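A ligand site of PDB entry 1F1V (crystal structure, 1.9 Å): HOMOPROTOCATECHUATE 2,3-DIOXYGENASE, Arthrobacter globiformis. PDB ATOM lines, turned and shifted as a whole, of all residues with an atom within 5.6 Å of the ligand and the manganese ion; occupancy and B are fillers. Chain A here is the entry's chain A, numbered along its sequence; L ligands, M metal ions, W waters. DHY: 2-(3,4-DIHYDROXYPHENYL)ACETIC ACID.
O2 of the ligand is in hydrogen-bond range of ND1 of His 248, 2.5 Å away. The side-chain hydroxyl (OH) of Tyr 257 lies close to an oxygen (O3) of the ligand (2.7 Å). An oxygen (O2) of the ligand sits close to the backbone carbonyl oxygen (O) of Arg 293 (2.8 Å). The guanidinium group (NH1) of Arg 293 is in salt-bridge range of an oxygen (O1) of the ligand (3.0 Å). The guanidinium group (NH1) of Arg 243 is in salt-bridge range of an oxygen (O1) of the ligand (2.9 Å). An oxygen (O4) of the ligand sits close to a ring nitrogen (NE2) of His 200, 3.3 Å away.
The side-chain carboxylate of Glu 267 lies within hydrogen-bond range of a ring nitrogen (NE2) of His 248 (2.9 Å). The side-chain carboxylate (OE2) of Glu 267 is in hydrogen-bond range of the side-chain hydroxyl (OH) of Tyr 257. A ring nitrogen (ND1) of His 155 sits close to a ring nitrogen (NE2) of His 200 (3.4 Å). O of His 155 is in hydrogen-bond range of N of Ala 216. A ring nitrogen (NE2) of His 248 sits close to the side-chain hydroxyl (OH) of Tyr 257 (3.4 Å). The backbone carbonyl oxygen (O) of Arg 293 sits close to a ring nitrogen (ND1) of His 248, at 3.5 Å. O of Arg 293 lies within hydrogen-bond range of N of Gly 249, 3.0 Å away. The guanidinium group (NH2) of Arg 243 is in hydrogen-bond range of the side-chain hydroxyl (OH) of Tyr 255.
Merely in contact with the ligand: Val 250 (3.2 Å), Ser 251 (3.3 Å), Trp 192 (3.4 Å), Trp 304 (3.5 Å), Tyr 269 (3.6 Å) and Asn 157 (3.97 Å). Hydrophobic or aromatic side chains within 4 Å of the ligand: His 155, Trp 192, His 200, His 214, His 248, Tyr 257, Tyr 269 and Trp 304. 14 residues have an atom within 4 Å of the ligand: His 155, Asn 157, Trp 192, His 200, His 214, Arg 243, His 248, Val 250, Ser 251, Tyr 257, Glu 267, Tyr 269, Arg 293 and Trp 304. The nearest printed residue that does not touch the ligand is Asp 294 (4.3 Å).
Residues that only touch the manganese ion: His 200 and Tyr 257. The nearest printed residue that does not touch the manganese ion is Ala 216 (4.5 Å).
The manganese ion is bound by O3 of the ligand (1.9 Å), OE1 of Glu 267 (2.0 Å), NE2 of His 155 (2.1 Å), O4 of the ligand (2.1 Å), NE2 of His 214 (2.2 Å) and water W1 (2.3 Å). The manganese ion has six donor atoms within binding distance.
Water W1 lies within hydrogen-bond range of NE2 of His 200 and ND2 of Asn 157.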
ATOM      1  N   HIS A 155     -14.115 -13.639  14.418  1.00  0.00           N
ATOM      2  CA  HIS A 155     -14.562 -12.875  15.610  1.00  0.00           C
ATOM      3  C   HIS A 155     -15.031 -13.743  16.776  1.00  0.00           C
ATOM      4  O   HIS A 155     -15.159 -15.002  16.677  1.00  0.00           O
ATOM      5  CB  HIS A 155     -15.733 -11.931  15.231  1.00  0.00           C
ATOM      6  CG  HIS A 155     -16.989 -12.659  14.786  1.00  0.00           C
ATOM      7  ND1 HIS A 155     -17.289 -12.878  13.452  1.00  0.00           N
ATOM      8  CD2 HIS A 155     -18.059 -13.120  15.478  1.00  0.00           C
ATOM      9  CE1 HIS A 155     -18.496 -13.429  13.349  1.00  0.00           C
ATOM     10  NE2 HIS A 155     -18.978 -13.578  14.570  1.00  0.00           N
ATOM     11  N   ASN A 157     -18.078 -13.637  20.093  1.00  0.00           N
ATOM     12  CA  ASN A 157     -19.315 -12.973  20.456  1.00  0.00           C
ATOM     13  C   ASN A 157     -19.498 -13.297  21.990  1.00  0.00           C
ATOM     14  O   ASN A 157     -19.363 -14.453  22.424  1.00  0.00           O
ATOM     15  CB  ASN A 157     -20.509 -13.477  19.656  1.00  0.00           C
ATOM     16  CG  ASN A 157     -21.752 -12.647  19.909  1.00  0.00           C
ATOM     17  OD1 ASN A 157     -22.157 -12.441  21.078  1.00  0.00           O
ATOM     18  ND2 ASN A 157     -22.362 -12.123  18.838  1.00  0.00           N
ATOM     19  N   TRP A 192     -21.653  -4.517  17.431  1.00  0.00           N
ATOM     20  CA  TRP A 192     -20.627  -5.211  16.689  1.00  0.00           C
ATOM     21  C   TRP A 192     -19.417  -4.273  16.676  1.00  0.00           C
ATOM     22  O   TRP A 192     -19.515  -3.139  16.179  1.00  0.00           O
ATOM     23  CB  TRP A 192     -21.170  -5.525  15.311  1.00  0.00           C
ATOM     24  CG  TRP A 192     -22.060  -6.740  15.358  1.00  0.00           C
ATOM     25  CD1 TRP A 192     -21.745  -8.034  14.914  1.00  0.00           C
ATOM     26  CD2 TRP A 192     -23.407  -6.807  15.851  1.00  0.00           C
ATOM     27  NE1 TRP A 192     -22.853  -8.872  15.116  1.00  0.00           N
ATOM     28  CE2 TRP A 192     -23.863  -8.141  15.685  1.00  0.00           C
ATOM     29  CE3 TRP A 192     -24.273  -5.866  16.413  1.00  0.00           C
ATOM     30  CZ2 TRP A 192     -25.151  -8.543  16.043  1.00  0.00           C
ATOM     31  CZ3 TRP A 192     -25.568  -6.269  16.779  1.00  0.00           C
ATOM     32  CH2 TRP A 192     -25.987  -7.599  16.593  1.00  0.00           C
ATOM     33  N   HIS A 200     -16.457  -6.992  12.512  1.00  0.00           N
ATOM     34  CA  HIS A 200     -16.118  -7.086  13.943  1.00  0.00           C
ATOM     35  C   HIS A 200     -15.049  -8.027  14.338  1.00  0.00           C
ATOM     36  O   HIS A 200     -14.772  -8.964  13.611  1.00  0.00           O
ATOM     37  CB  HIS A 200     -17.360  -7.396  14.808  1.00  0.00           C
ATOM     38  CG  HIS A 200     -18.061  -8.711  14.512  1.00  0.00           C
ATOM     39  ND1 HIS A 200     -18.421  -9.108  13.253  1.00  0.00           N
ATOM     40  CD2 HIS A 200     -18.684  -9.590  15.353  1.00  0.00           C
ATOM     41  CE1 HIS A 200     -19.245 -10.145  13.313  1.00  0.00           C
ATOM     42  NE2 HIS A 200     -19.427 -10.459  14.575  1.00  0.00           N
ATOM     43  N   HIS A 214     -20.217 -17.363  20.994  1.00  0.00           N
ATOM     44  CA  HIS A 214     -19.619 -18.142  19.940  1.00  0.00           C
ATOM     45  C   HIS A 214     -18.294 -17.565  19.458  1.00  0.00           C
ATOM     46  O   HIS A 214     -17.948 -16.400  19.734  1.00  0.00           O
ATOM     47  CB  HIS A 214     -20.559 -18.275  18.719  1.00  0.00           C
ATOM     48  CG  HIS A 214     -20.873 -16.996  18.037  1.00  0.00           C
ATOM     49  ND1 HIS A 214     -21.978 -16.231  18.357  1.00  0.00           N
ATOM     50  CD2 HIS A 214     -20.265 -16.368  16.989  1.00  0.00           C
ATOM     51  CE1 HIS A 214     -22.048 -15.195  17.532  1.00  0.00           C
ATOM     52  NE2 HIS A 214     -21.025 -15.249  16.696  1.00  0.00           N
ATOM     53  N   ALA A 216     -16.159 -17.431  15.702  1.00  0.00           N
ATOM     54  CA  ALA A 216     -16.517 -17.557  14.269  1.00  0.00           C
ATOM     55  C   ALA A 216     -15.338 -17.696  13.322  1.00  0.00           C
ATOM     56  O   ALA A 216     -14.305 -16.966  13.435  1.00  0.00           O
ATOM     57  CB  ALA A 216     -17.317 -16.320  13.829  1.00  0.00           C
ATOM     58  N   ARG A 243     -28.601 -23.375  14.085  1.00  0.00           N
ATOM     59  CA  ARG A 243     -29.307 -22.295  13.441  1.00  0.00           C
ATOM     60  C   ARG A 243     -28.670 -22.023  12.091  1.00  0.00           C
ATOM     61  O   ARG A 243     -27.427 -22.015  11.988  1.00  0.00           O
ATOM     62  CB  ARG A 243     -29.215 -21.035  14.329  1.00  0.00           C
ATOM     63  CG  ARG A 243     -29.843 -19.815  13.732  1.00  0.00           C
ATOM     64  CD  ARG A 243     -29.762 -18.562  14.622  1.00  0.00           C
ATOM     65  NE  ARG A 243     -30.108 -17.414  13.800  1.00  0.00           N
ATOM     66  CZ  ARG A 243     -29.719 -16.164  14.004  1.00  0.00           C
ATOM     67  NH1 ARG A 243     -28.961 -15.821  15.037  1.00  0.00           N
ATOM     68  NH2 ARG A 243     -30.053 -15.230  13.126  1.00  0.00           N
ATOM     69  N   HIS A 248     -27.476 -12.925   7.506  1.00  0.00           N
ATOM     70  CA  HIS A 248     -27.644 -11.992   8.635  1.00  0.00           C
ATOM     71  C   HIS A 248     -28.093 -10.606   8.074  1.00  0.00           C
ATOM     72  O   HIS A 248     -27.590 -10.173   7.014  1.00  0.00           O
ATOM     73  CB  HIS A 248     -26.290 -11.686   9.315  1.00  0.00           C
ATOM     74  CG  HIS A 248     -25.790 -12.747  10.236  1.00  0.00           C
ATOM     75  ND1 HIS A 248     -26.542 -13.230  11.291  1.00  0.00           N
ATOM     76  CD2 HIS A 248     -24.593 -13.392  10.291  1.00  0.00           C
ATOM     77  CE1 HIS A 248     -25.834 -14.126  11.944  1.00  0.00           C
ATOM     78  NE2 HIS A 248     -24.647 -14.240  11.364  1.00  0.00           N
ATOM     79  N   GLY A 249     -28.948  -9.892   8.798  1.00  0.00           N
ATOM     80  CA  GLY A 249     -29.278  -8.531   8.399  1.00  0.00           C
ATOM     81  C   GLY A 249     -28.028  -7.768   8.842  1.00  0.00           C
ATOM     82  O   GLY A 249     -27.278  -7.254   8.008  1.00  0.00           O
ATOM     83  N   VAL A 250     -27.814  -7.665  10.178  1.00  0.00           N
ATOM     84  CA  VAL A 250     -26.588  -7.033  10.734  1.00  0.00           C
ATOM     85  C   VAL A 250     -25.359  -7.823  10.185  1.00  0.00           C
ATOM     86  O   VAL A 250     -25.343  -9.065  10.263  1.00  0.00           O
ATOM     87  CB  VAL A 250     -26.552  -7.176  12.301  1.00  0.00           C
ATOM     88  CG1 VAL A 250     -25.166  -6.716  12.850  1.00  0.00           C
ATOM     89  CG2 VAL A 250     -27.702  -6.403  12.909  1.00  0.00           C
ATOM     90  N   SER A 251     -24.383  -7.115   9.639  1.00  0.00           N
ATOM     91  CA  SER A 251     -23.154  -7.662   9.062  1.00  0.00           C
ATOM     92  C   SER A 251     -23.290  -8.122   7.621  1.00  0.00           C
ATOM     93  O   SER A 251     -22.293  -8.114   6.877  1.00  0.00           O
ATOM     94  CB  SER A 251     -22.584  -8.835   9.912  1.00  0.00           C
ATOM     95  OG  SER A 251     -23.155 -10.105   9.550  1.00  0.00           O
ATOM     96  N   TYR A 255     -24.345 -17.225   7.026  1.00  0.00           N
ATOM     97  CA  TYR A 255     -23.924 -17.875   8.263  1.00  0.00           C
ATOM     98  C   TYR A 255     -24.459 -19.226   8.598  1.00  0.00           C
ATOM     99  O   TYR A 255     -25.535 -19.637   8.070  1.00  0.00           O
ATOM    100  CB  TYR A 255     -24.283 -16.968   9.472  1.00  0.00           C
ATOM    101  CG  TYR A 255     -25.775 -16.960   9.783  1.00  0.00           C
ATOM    102  CD1 TYR A 255     -26.363 -18.000  10.515  1.00  0.00           C
ATOM    103  CD2 TYR A 255     -26.609 -15.966   9.271  1.00  0.00           C
ATOM    104  CE1 TYR A 255     -27.752 -18.063  10.709  1.00  0.00           C
ATOM    105  CE2 TYR A 255     -27.986 -16.008   9.464  1.00  0.00           C
ATOM    106  CZ  TYR A 255     -28.555 -17.053  10.186  1.00  0.00           C
ATOM    107  OH  TYR A 255     -29.919 -17.044  10.452  1.00  0.00           O
ATOM    108  N   TYR A 257     -24.538 -21.798  12.401  1.00  0.00           N
ATOM    109  CA  TYR A 257     -24.126 -22.056  13.784  1.00  0.00           C
ATOM    110  C   TYR A 257     -24.244 -23.530  14.110  1.00  0.00           C
ATOM    111  O   TYR A 257     -25.335 -24.092  13.934  1.00  0.00           O
ATOM    112  CB  TYR A 257     -25.020 -21.304  14.793  1.00  0.00           C
ATOM    113  CG  TYR A 257     -24.863 -19.807  14.698  1.00  0.00           C
ATOM    114  CD1 TYR A 257     -23.788 -19.135  15.324  1.00  0.00           C
ATOM    115  CD2 TYR A 257     -25.792 -19.046  13.974  1.00  0.00           C
ATOM    116  CE1 TYR A 257     -23.678 -17.733  15.244  1.00  0.00           C
ATOM    117  CE2 TYR A 257     -25.659 -17.628  13.889  1.00  0.00           C
ATOM    118  CZ  TYR A 257     -24.613 -17.001  14.524  1.00  0.00           C
ATOM    119  OH  TYR A 257     -24.552 -15.620  14.423  1.00  0.00           O
ATOM    120  N   GLU A 267     -19.532 -20.497  14.828  1.00  0.00           N
ATOM    121  CA  GLU A 267     -20.218 -19.932  13.663  1.00  0.00           C
ATOM    122  C   GLU A 267     -19.301 -20.084  12.456  1.00  0.00           C
ATOM    123  O   GLU A 267     -18.082 -19.963  12.605  1.00  0.00           O
ATOM    124  CB  GLU A 267     -20.531 -18.452  13.856  1.00  0.00           C
ATOM    125  CG  GLU A 267     -21.214 -17.806  12.662  1.00  0.00           C
ATOM    126  CD  GLU A 267     -21.485 -16.343  12.892  1.00  0.00           C
ATOM    127  OE1 GLU A 267     -20.890 -15.764  13.855  1.00  0.00           O
ATOM    128  OE2 GLU A 267     -22.289 -15.773  12.125  1.00  0.00           O
ATOM    129  N   TYR A 269     -18.940 -18.418   8.786  1.00  0.00           N
ATOM    130  CA  TYR A 269     -19.382 -17.121   8.275  1.00  0.00           C
ATOM    131  C   TYR A 269     -18.698 -16.767   6.963  1.00  0.00           C
ATOM    132  O   TYR A 269     -17.554 -17.115   6.769  1.00  0.00           O
ATOM    133  CB  TYR A 269     -18.871 -16.167   9.381  1.00  0.00           C
ATOM    134  CG  TYR A 269     -19.027 -14.700   9.279  1.00  0.00           C
ATOM    135  CD1 TYR A 269     -18.086 -13.881   8.590  1.00  0.00           C
ATOM    136  CD2 TYR A 269     -20.038 -14.064  10.042  1.00  0.00           C
ATOM    137  CE1 TYR A 269     -18.157 -12.471   8.684  1.00  0.00           C
ATOM    138  CE2 TYR A 269     -20.117 -12.677  10.154  1.00  0.00           C
ATOM    139  CZ  TYR A 269     -19.196 -11.875   9.486  1.00  0.00           C
ATOM    140  OH  TYR A 269     -19.332 -10.511   9.679  1.00  0.00           O
ATOM    141  N   ARG A 292     -33.348  -7.772  11.139  1.00  0.00           N
ATOM    142  CA  ARG A 292     -32.039  -7.434  11.671  1.00  0.00           C
ATOM    143  C   ARG A 292     -31.202  -8.661  12.010  1.00  0.00           C
ATOM    144  O   ARG A 292     -29.975  -8.595  11.981  1.00  0.00           O
ATOM    145  CB  ARG A 292     -32.140  -6.537  12.914  1.00  0.00           C
ATOM    146  CG  ARG A 292     -32.660  -7.270  14.143  1.00  0.00           C
ATOM    147  CD  ARG A 292     -33.099  -6.329  15.254  1.00  0.00           C
ATOM    148  NE  ARG A 292     -34.095  -7.029  16.029  1.00  0.00           N
ATOM    149  CZ  ARG A 292     -33.835  -7.835  17.057  1.00  0.00           C
ATOM    150  NH1 ARG A 292     -32.590  -8.029  17.482  1.00  0.00           N
ATOM    151  NH2 ARG A 292     -34.831  -8.523  17.614  1.00  0.00           N
ATOM    152  N   ARG A 293     -31.828  -9.780  12.341  1.00  0.00           N
ATOM    153  CA  ARG A 293     -31.018 -10.932  12.704  1.00  0.00           C
ATOM    154  C   ARG A 293     -30.864 -11.783  11.447  1.00  0.00           C
ATOM    155  O   ARG A 293     -29.756 -11.938  10.898  1.00  0.00           O
ATOM    156  CB  ARG A 293     -31.683 -11.739  13.844  1.00  0.00           C
ATOM    157  CG  ARG A 293     -31.712 -11.023  15.229  1.00  0.00           C
ATOM    158  CD  ARG A 293     -30.682 -11.588  16.261  1.00  0.00           C
ATOM    159  NE  ARG A 293     -30.507 -10.790  17.503  1.00  0.00           N
ATOM    160  CZ  ARG A 293     -29.312 -10.579  18.078  1.00  0.00           C
ATOM    161  NH1 ARG A 293     -28.216 -11.111  17.531  1.00  0.00           N
ATOM    162  NH2 ARG A 293     -29.200  -9.835  19.187  1.00  0.00           N
ATOM    163  N   ASP A 294     -32.000 -12.280  10.990  1.00  0.00           N
ATOM    164  CA  ASP A 294     -32.058 -13.078   9.789  1.00  0.00           C
ATOM    165  C   ASP A 294     -32.815 -12.280   8.694  1.00  0.00           C
ATOM    166  O   ASP A 294     -34.014 -11.980   8.777  1.00  0.00           O
ATOM    167  CB  ASP A 294     -32.703 -14.418  10.118  1.00  0.00           C
ATOM    168  CG  ASP A 294     -32.655 -15.367   8.971  1.00  0.00           C
ATOM    169  OD1 ASP A 294     -33.578 -15.254   8.110  1.00  0.00           O
ATOM    170  OD2 ASP A 294     -31.712 -16.200   8.905  1.00  0.00           O
ATOM    171  N   TRP A 304     -30.512 -20.326  21.061  1.00  0.00           N
ATOM    172  CA  TRP A 304     -29.515 -19.383  20.589  1.00  0.00           C
ATOM    173  C   TRP A 304     -29.431 -18.172  21.546  1.00  0.00           C
ATOM    174  O   TRP A 304     -28.374 -17.556  21.669  1.00  0.00           O
ATOM    175  CB  TRP A 304     -29.863 -18.925  19.137  1.00  0.00           C
ATOM    176  CG  TRP A 304     -28.705 -18.253  18.414  1.00  0.00           C
ATOM    177  CD1 TRP A 304     -27.767 -18.861  17.627  1.00  0.00           C
ATOM    178  CD2 TRP A 304     -28.348 -16.876  18.451  1.00  0.00           C
ATOM    179  NE1 TRP A 304     -26.867 -17.941  17.145  1.00  0.00           N
ATOM    180  CE2 TRP A 304     -27.205 -16.701  17.643  1.00  0.00           C
ATOM    181  CE3 TRP A 304     -28.895 -15.754  19.084  1.00  0.00           C
ATOM    182  CZ2 TRP A 304     -26.588 -15.481  17.452  1.00  0.00           C
ATOM    183  CZ3 TRP A 304     -28.280 -14.528  18.906  1.00  0.00           C
ATOM    184  CH2 TRP A 304     -27.136 -14.396  18.094  1.00  0.00           C
HETATM  185  C1  DHY L   1     -25.657 -11.455  14.019  1.00  0.00           C
HETATM  186  C2  DHY L   1     -24.993 -12.430  14.829  1.00  0.00           C
HETATM  187  C3  DHY L   1     -23.654 -12.789  14.581  1.00  0.00           C
HETATM  188  C4  DHY L   1     -22.932 -12.134  13.505  1.00  0.00           C
HETATM  189  C5  DHY L   1     -23.578 -11.137  12.687  1.00  0.00           C
HETATM  190  C6  DHY L   1     -24.937 -10.794  12.955  1.00  0.00           C
HETATM  191  C7  DHY L   1     -27.062 -11.200  14.384  1.00  0.00           C
HETATM  192  C8  DHY L   1     -27.968 -12.378  14.160  1.00  0.00           C
HETATM  193  O1  DHY L   1     -28.448 -12.955  15.156  1.00  0.00           O
HETATM  194  O2  DHY L   1     -28.284 -12.895  13.066  1.00  0.00           O
HETATM  195  O3  DHY L   1     -22.853 -13.747  15.246  1.00  0.00           O
HETATM  196  O4  DHY L   1     -21.587 -12.612  13.401  1.00  0.00           O
HETATM  197 MN    MN M   1     -21.021 -14.046  14.875  1.00  0.00          MN
HETATM  198  O   HOH W   1     -21.133 -12.109  16.158  1.00  0.00           O
